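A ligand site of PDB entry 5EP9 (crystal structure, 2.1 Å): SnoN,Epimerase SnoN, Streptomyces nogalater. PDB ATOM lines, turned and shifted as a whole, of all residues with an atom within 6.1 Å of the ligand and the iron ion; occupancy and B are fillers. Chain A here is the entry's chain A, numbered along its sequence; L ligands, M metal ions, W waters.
O5 of the ligand sits at hydrogen-bond distance from OG1 of Thr 139.
NH2 of Arg 236 lies within salt-bridge range of O4 of the ligand, at 2.8 Å.
An oxygen (O4) of the ligand sits at hydrogen-bond distance from the indole nitrogen (NE1) of Trp 160.
The side-chain hydroxyl (OG) of Ser 240 is in hydrogen-bond range of an oxygen (O2) of the ligand.
A ring nitrogen (NE2) of His 219 lies close to an oxygen (O1) of the ligand (3.2 Å).
A ring nitrogen (NE2) of His 219 sits at hydrogen-bond distance from the side-chain carboxylate (OD2) of Asp 144 (2.8 Å).
NE2 of His 225 sits close to NE2 of His 219 (3.2 Å).
The backbone carbonyl oxygen of Ala 227 sits at hydrogen-bond distance from the backbone NH of Thr 139, at 2.8 Å.
The side-chain hydroxyl of Thr 139 is in hydrogen-bond range of the side-chain amino group of Lys 128, 2.9 Å away.
N of Arg 236 lies within hydrogen-bond range of O of Lys 128 (2.8 Å).
O of Gly 171 is in hydrogen-bond range of NH1 of Arg 236 (2.9 Å).
The backbone carbonyl oxygen of His 219 lies within hydrogen-bond range of the backbone NH of Thr 158, at 2.9 Å.
The backbone NH (N) of Leu 126 sits at hydrogen-bond distance from the backbone carbonyl oxygen (O) of Ser 238.
Met 84 touches the ligand.
Leu 126 touches the ligand.
Lys 128 touches the ligand.
Thr 158 touches the ligand (CG2 to O2, 3.7 Å).
Met 173 touches the ligand (SD to C3, 3.7 Å).
CB of Ala 227 touches O5 of the ligand, at 3.3 Å.
Hydrophobic or aromatic side chains that line the ligand: Met 84, Leu 126, His 142, Trp 160, Met 173, His 219, His 225 and Ala 227.
Within 4 Å of the ligand: Met 84, Leu 126, Lys 128, Thr 139, His 142, Asp 144, Thr 158, Trp 160, Met 173, His 219, His 225, Ala 227, Arg 236 and Ser 240.
Three residues have an atom within 4 Å of the iron ion: His 142, Asp 144 and His 225.
O3 of the ligand is bound to the iron ion, 1.9 Å away.
OD1 of Asp 144 binds the iron ion.
The iron ion is bound by water W2.
O1 of the ligand is bound to the iron ion.
A ring nitrogen (NE2) of His 225 binds the iron ion (2.1 Å).
A ring nitrogen (NE2) of His 142 binds the iron ion, 2.2 Å away.
Water W1 lies within hydrogen-bond range of OG1 of Thr 158 (2.6 Å) and OD2 of Asp 144 (3.0 Å).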
ATOM      1  N   TRP A  76     -31.603  -8.852  29.880  1.00  0.00           N
ATOM      2  CA  TRP A  76     -31.383  -9.112  28.467  1.00  0.00           C
ATOM      3  C   TRP A  76     -30.116  -9.969  28.299  1.00  0.00           C
ATOM      4  O   TRP A  76     -28.973  -9.521  28.428  1.00  0.00           O
ATOM      5  CB  TRP A  76     -31.255  -7.819  27.663  1.00  0.00           C
ATOM      6  CG  TRP A  76     -31.094  -7.962  26.116  1.00  0.00           C
ATOM      7  CD1 TRP A  76     -31.112  -9.119  25.380  1.00  0.00           C
ATOM      8  CD2 TRP A  76     -30.901  -6.893  25.166  1.00  0.00           C
ATOM      9  NE1 TRP A  76     -30.941  -8.823  24.041  1.00  0.00           N
ATOM     10  CE2 TRP A  76     -30.808  -7.473  23.879  1.00  0.00           C
ATOM     11  CE3 TRP A  76     -30.827  -5.510  25.271  1.00  0.00           C
ATOM     12  CZ2 TRP A  76     -30.603  -6.695  22.710  1.00  0.00           C
ATOM     13  CZ3 TRP A  76     -30.645  -4.700  24.114  1.00  0.00           C
ATOM     14  CH2 TRP A  76     -30.527  -5.300  22.845  1.00  0.00           C
ATOM     15  N   VAL A  83     -26.122  -9.217  28.151  1.00  0.00           N
ATOM     16  CA  VAL A  83     -26.094  -8.028  27.348  1.00  0.00           C
ATOM     17  C   VAL A  83     -26.288  -6.849  28.268  1.00  0.00           C
ATOM     18  O   VAL A  83     -25.559  -5.860  28.191  1.00  0.00           O
ATOM     19  CB  VAL A  83     -27.181  -8.050  26.244  1.00  0.00           C
ATOM     20  CG1 VAL A  83     -27.110  -6.800  25.445  1.00  0.00           C
ATOM     21  CG2 VAL A  83     -27.017  -9.267  25.277  1.00  0.00           C
ATOM     22  N   MET A  84     -27.300  -6.939  29.103  1.00  0.00           N
ATOM     23  CA  MET A  84     -27.609  -5.895  30.071  1.00  0.00           C
ATOM     24  C   MET A  84     -28.696  -6.299  31.068  1.00  0.00           C
ATOM     25  O   MET A  84     -29.442  -7.226  30.831  1.00  0.00           O
ATOM     26  CB  MET A  84     -28.081  -4.591  29.415  1.00  0.00           C
ATOM     27  CG  MET A  84     -29.361  -4.741  28.612  1.00  0.00           C
ATOM     28  SD  MET A  84     -29.795  -3.055  28.027  1.00  0.00           S
ATOM     29  CE  MET A  84     -28.525  -2.761  26.791  1.00  0.00           C
ATOM     30  N   LEU A 126     -30.507   1.527  32.127  1.00  0.00           N
ATOM     31  CA  LEU A 126     -29.658   0.466  31.586  1.00  0.00           C
ATOM     32  C   LEU A 126     -28.425   0.283  32.419  1.00  0.00           C
ATOM     33  O   LEU A 126     -27.803   1.239  32.791  1.00  0.00           O
ATOM     34  CB  LEU A 126     -29.257   0.701  30.135  1.00  0.00           C
ATOM     35  CG  LEU A 126     -30.385   1.093  29.191  1.00  0.00           C
ATOM     36  CD1 LEU A 126     -29.824   1.325  27.798  1.00  0.00           C
ATOM     37  CD2 LEU A 126     -31.439   0.031  29.121  1.00  0.00           C
ATOM     38  N   LYS A 128     -24.851  -2.191  32.332  1.00  0.00           N
ATOM     39  CA  LYS A 128     -23.870  -3.212  31.981  1.00  0.00           C
ATOM     40  C   LYS A 128     -22.780  -3.246  32.964  1.00  0.00           C
ATOM     41  O   LYS A 128     -22.140  -2.266  33.248  1.00  0.00           O
ATOM     42  CB  LYS A 128     -23.155  -2.965  30.635  1.00  0.00           C
ATOM     43  CG  LYS A 128     -23.927  -3.208  29.420  1.00  0.00           C
ATOM     44  CD  LYS A 128     -22.914  -3.191  28.229  1.00  0.00           C
ATOM     45  CE  LYS A 128     -23.651  -3.200  26.905  1.00  0.00           C
ATOM     46  NZ  LYS A 128     -23.842  -4.560  26.361  1.00  0.00           N
ATOM     47  N   THR A 139     -23.640  -5.385  23.137  1.00  0.00           N
ATOM     48  CA  THR A 139     -24.939  -5.271  22.540  1.00  0.00           C
ATOM     49  C   THR A 139     -24.762  -5.432  21.008  1.00  0.00           C
ATOM     50  O   THR A 139     -24.180  -4.570  20.399  1.00  0.00           O
ATOM     51  CB  THR A 139     -25.558  -3.878  22.827  1.00  0.00           C
ATOM     52  OG1 THR A 139     -25.662  -3.689  24.228  1.00  0.00           O
ATOM     53  CG2 THR A 139     -26.989  -3.872  22.306  1.00  0.00           C
ATOM     54  N   HIS A 142     -28.111  -3.572  15.700  1.00  0.00           N
ATOM     55  CA  HIS A 142     -29.484  -3.644  15.351  1.00  0.00           C
ATOM     56  C   HIS A 142     -29.953  -2.252  15.010  1.00  0.00           C
ATOM     57  O   HIS A 142     -29.277  -1.264  15.277  1.00  0.00           O
ATOM     58  CB  HIS A 142     -30.273  -4.228  16.512  1.00  0.00           C
ATOM     59  CG  HIS A 142     -30.268  -3.342  17.728  1.00  0.00           C
ATOM     60  ND1 HIS A 142     -29.198  -3.264  18.556  1.00  0.00           N
ATOM     61  CD2 HIS A 142     -31.150  -2.434  18.187  1.00  0.00           C
ATOM     62  CE1 HIS A 142     -29.429  -2.393  19.518  1.00  0.00           C
ATOM     63  NE2 HIS A 142     -30.635  -1.921  19.355  1.00  0.00           N
ATOM     64  N   HIS A 143     -31.155  -2.171  14.504  1.00  0.00           N
ATOM     65  CA  HIS A 143     -31.925  -0.919  14.542  1.00  0.00           C
ATOM     66  C   HIS A 143     -33.191  -1.059  15.309  1.00  0.00           C
ATOM     67  O   HIS A 143     -33.623  -2.126  15.532  1.00  0.00           O
ATOM     68  CB  HIS A 143     -32.177  -0.280  13.200  1.00  0.00           C
ATOM     69  CG  HIS A 143     -32.969  -1.088  12.277  1.00  0.00           C
ATOM     70  ND1 HIS A 143     -32.419  -2.110  11.551  1.00  0.00           N
ATOM     71  CD2 HIS A 143     -34.255  -0.974  11.880  1.00  0.00           C
ATOM     72  CE1 HIS A 143     -33.328  -2.575  10.722  1.00  0.00           C
ATOM     73  NE2 HIS A 143     -34.460  -1.894  10.902  1.00  0.00           N
ATOM     74  N   ASP A 144     -33.731   0.035  15.805  1.00  0.00           N
ATOM     75  CA  ASP A 144     -34.726  -0.114  16.884  1.00  0.00           C
ATOM     76  C   ASP A 144     -36.149  -0.238  16.350  1.00  0.00           C
ATOM     77  O   ASP A 144     -37.014  -0.804  17.006  1.00  0.00           O
ATOM     78  CB  ASP A 144     -34.661   1.129  17.855  1.00  0.00           C
ATOM     79  CG  ASP A 144     -33.410   1.260  18.580  1.00  0.00           C
ATOM     80  OD1 ASP A 144     -32.825   0.238  19.043  1.00  0.00           O
ATOM     81  OD2 ASP A 144     -33.059   2.437  18.810  1.00  0.00           O
ATOM     82  N   THR A 158     -34.306   7.911  19.926  1.00  0.00           N
ATOM     83  CA  THR A 158     -33.910   7.499  21.240  1.00  0.00           C
ATOM     84  C   THR A 158     -32.831   8.460  21.831  1.00  0.00           C
ATOM     85  O   THR A 158     -31.870   8.726  21.192  1.00  0.00           O
ATOM     86  CB  THR A 158     -33.423   6.070  21.211  1.00  0.00           C
ATOM     87  OG1 THR A 158     -34.482   5.204  20.810  1.00  0.00           O
ATOM     88  CG2 THR A 158     -32.862   5.647  22.567  1.00  0.00           C
ATOM     89  N   TRP A 160     -30.066   8.627  24.697  1.00  0.00           N
ATOM     90  CA  TRP A 160     -29.305   7.745  25.566  1.00  0.00           C
ATOM     91  C   TRP A 160     -28.417   8.650  26.398  1.00  0.00           C
ATOM     92  O   TRP A 160     -27.543   9.338  25.867  1.00  0.00           O
ATOM     93  CB  TRP A 160     -28.472   6.790  24.713  1.00  0.00           C
ATOM     94  CG  TRP A 160     -27.845   5.557  25.318  1.00  0.00           C
ATOM     95  CD1 TRP A 160     -28.268   4.270  25.135  1.00  0.00           C
ATOM     96  CD2 TRP A 160     -26.645   5.488  26.072  1.00  0.00           C
ATOM     97  NE1 TRP A 160     -27.406   3.408  25.745  1.00  0.00           N
ATOM     98  CE2 TRP A 160     -26.452   4.130  26.399  1.00  0.00           C
ATOM     99  CE3 TRP A 160     -25.816   6.472  26.662  1.00  0.00           C
ATOM    100  CZ2 TRP A 160     -25.376   3.695  27.130  1.00  0.00           C
ATOM    101  CZ3 TRP A 160     -24.706   6.034  27.450  1.00  0.00           C
ATOM    102  CH2 TRP A 160     -24.495   4.647  27.647  1.00  0.00           C
ATOM    103  N   GLY A 171     -18.238   0.260  27.458  1.00  0.00           N
ATOM    104  CA  GLY A 171     -19.356  -0.169  26.598  1.00  0.00           C
ATOM    105  C   GLY A 171     -20.122   0.919  25.912  1.00  0.00           C
ATOM    106  O   GLY A 171     -21.367   0.893  25.910  1.00  0.00           O
ATOM    107  N   MET A 173     -21.492   3.261  22.836  1.00  0.00           N
ATOM    108  CA  MET A 173     -22.167   2.873  21.560  1.00  0.00           C
ATOM    109  C   MET A 173     -21.335   3.166  20.316  1.00  0.00           C
ATOM    110  O   MET A 173     -20.518   4.074  20.317  1.00  0.00           O
ATOM    111  CB  MET A 173     -23.558   3.490  21.445  1.00  0.00           C
ATOM    112  CG  MET A 173     -24.483   2.974  22.580  1.00  0.00           C
ATOM    113  SD  MET A 173     -26.231   2.831  22.114  1.00  0.00           S
ATOM    114  CE  MET A 173     -26.504   4.515  22.374  1.00  0.00           C
ATOM    115  N   HIS A 219     -30.358   8.971  18.672  1.00  0.00           N
ATOM    116  CA  HIS A 219     -30.327   8.195  17.421  1.00  0.00           C
ATOM    117  C   HIS A 219     -31.701   7.864  16.868  1.00  0.00           C
ATOM    118  O   HIS A 219     -32.639   7.447  17.578  1.00  0.00           O
ATOM    119  CB  HIS A 219     -29.402   6.969  17.529  1.00  0.00           C
ATOM    120  CG  HIS A 219     -29.917   5.875  18.366  1.00  0.00           C
ATOM    121  ND1 HIS A 219     -29.687   5.818  19.731  1.00  0.00           N
ATOM    122  CD2 HIS A 219     -30.576   4.740  18.052  1.00  0.00           C
ATOM    123  CE1 HIS A 219     -30.177   4.686  20.202  1.00  0.00           C
ATOM    124  NE2 HIS A 219     -30.735   4.031  19.222  1.00  0.00           N
ATOM    125  N   HIS A 225     -26.870   0.457  15.266  1.00  0.00           N
ATOM    126  CA  HIS A 225     -26.074   0.763  16.410  1.00  0.00           C
ATOM    127  C   HIS A 225     -25.824  -0.487  17.218  1.00  0.00           C
ATOM    128  O   HIS A 225     -26.519  -1.482  17.146  1.00  0.00           O
ATOM    129  CB  HIS A 225     -26.651   1.855  17.301  1.00  0.00           C
ATOM    130  CG  HIS A 225     -28.048   1.559  17.821  1.00  0.00           C
ATOM    131  ND1 HIS A 225     -29.119   1.575  16.980  1.00  0.00           N
ATOM    132  CD2 HIS A 225     -28.504   1.175  19.020  1.00  0.00           C
ATOM    133  CE1 HIS A 225     -30.192   1.192  17.658  1.00  0.00           C
ATOM    134  NE2 HIS A 225     -29.862   1.013  18.917  1.00  0.00           N
ATOM    135  N   SER A 226     -24.740  -0.416  17.961  1.00  0.00           N
ATOM    136  CA  SER A 226     -24.313  -1.491  18.834  1.00  0.00           C
ATOM    137  C   SER A 226     -23.618  -0.891  20.044  1.00  0.00           C
ATOM    138  O   SER A 226     -23.454   0.314  20.138  1.00  0.00           O
ATOM    139  CB  SER A 226     -23.308  -2.401  18.076  1.00  0.00           C
ATOM    140  OG  SER A 226     -22.106  -1.746  17.874  1.00  0.00           O
ATOM    141  N   ALA A 227     -23.085  -1.742  20.914  1.00  0.00           N
ATOM    142  CA  ALA A 227     -22.341  -1.263  22.048  1.00  0.00           C
ATOM    143  C   ALA A 227     -21.384  -2.309  22.489  1.00  0.00           C
ATOM    144  O   ALA A 227     -21.660  -3.532  22.384  1.00  0.00           O
ATOM    145  CB  ALA A 227     -23.282  -0.871  23.237  1.00  0.00           C
ATOM    146  N   GLY A 228     -20.290  -1.842  23.057  1.00  0.00           N
ATOM    147  CA  GLY A 228     -19.251  -2.789  23.553  1.00  0.00           C
ATOM    148  C   GLY A 228     -19.684  -3.449  24.840  1.00  0.00           C
ATOM    149  O   GLY A 228     -20.664  -3.066  25.503  1.00  0.00           O
ATOM    150  N   ARG A 236     -21.598   0.433  33.939  1.00  0.00           N
ATOM    151  CA  ARG A 236     -22.063   1.364  32.931  1.00  0.00           C
ATOM    152  C   ARG A 236     -23.559   1.645  33.282  1.00  0.00           C
ATOM    153  O   ARG A 236     -24.383   0.734  33.269  1.00  0.00           O
ATOM    154  CB  ARG A 236     -21.989   0.783  31.536  1.00  0.00           C
ATOM    155  CG  ARG A 236     -22.182   1.852  30.478  1.00  0.00           C
ATOM    156  CD  ARG A 236     -22.526   1.254  29.146  1.00  0.00           C
ATOM    157  NE  ARG A 236     -23.901   0.805  29.092  1.00  0.00           N
ATOM    158  CZ  ARG A 236     -24.505   0.283  28.042  1.00  0.00           C
ATOM    159  NH1 ARG A 236     -23.881  -0.013  26.911  1.00  0.00           N
ATOM    160  NH2 ARG A 236     -25.766  -0.049  28.145  1.00  0.00           N
ATOM    161  N   SER A 238     -26.930   4.316  32.563  1.00  0.00           N
ATOM    162  CA  SER A 238     -27.470   5.284  31.631  1.00  0.00           C
ATOM    163  C   SER A 238     -28.944   5.120  31.600  1.00  0.00           C
ATOM    164  O   SER A 238     -29.489   4.101  32.102  1.00  0.00           O
ATOM    165  CB  SER A 238     -26.895   5.046  30.191  1.00  0.00           C
ATOM    166  OG  SER A 238     -27.176   3.724  29.742  1.00  0.00           O
ATOM    167  N   SER A 240     -32.209   5.275  28.603  1.00  0.00           N
ATOM    168  CA  SER A 240     -32.619   5.295  27.206  1.00  0.00           C
ATOM    169  C   SER A 240     -34.094   5.541  27.071  1.00  0.00           C
ATOM    170  O   SER A 240     -34.906   4.805  27.597  1.00  0.00           O
ATOM    171  CB  SER A 240     -32.211   3.954  26.556  1.00  0.00           C
ATOM    172  OG  SER A 240     -32.330   4.020  25.206  1.00  0.00           O
HETATM  173  C1  LIG L   1     -30.807   1.730  22.264  1.00  0.00           C
HETATM  174  O1  LIG L   1     -31.598   1.734  21.288  1.00  0.00           O
HETATM  175  O2  LIG L   1     -30.764   2.678  23.091  1.00  0.00           O
HETATM  176  C2  LIG L   1     -29.827   0.627  22.417  1.00  0.00           C
HETATM  177  O3  LIG L   1     -29.840  -0.313  21.595  1.00  0.00           O
HETATM  178  C3  LIG L   1     -28.865   0.687  23.628  1.00  0.00           C
HETATM  179  C4  LIG L   1     -27.764  -0.356  23.669  1.00  0.00           C
HETATM  180  C5  LIG L   1     -26.841  -0.316  24.868  1.00  0.00           C
HETATM  181  O4  LIG L   1     -26.966   0.607  25.694  1.00  0.00           O
HETATM  182  O5  LIG L   1     -25.984  -1.231  25.042  1.00  0.00           O
HETATM  183 FE    FE M   1     -31.188  -0.006  20.228  1.00  0.00          FE
HETATM  184  O   HOH W   1     -34.159   2.690  21.563  1.00  0.00           O
HETATM  185  O   HOH W   2     -32.377  -1.009  21.605  1.00  0.00           O
HETATM  186  O   HOH W   3     -31.875  -0.635  24.100  1.00  0.00           O
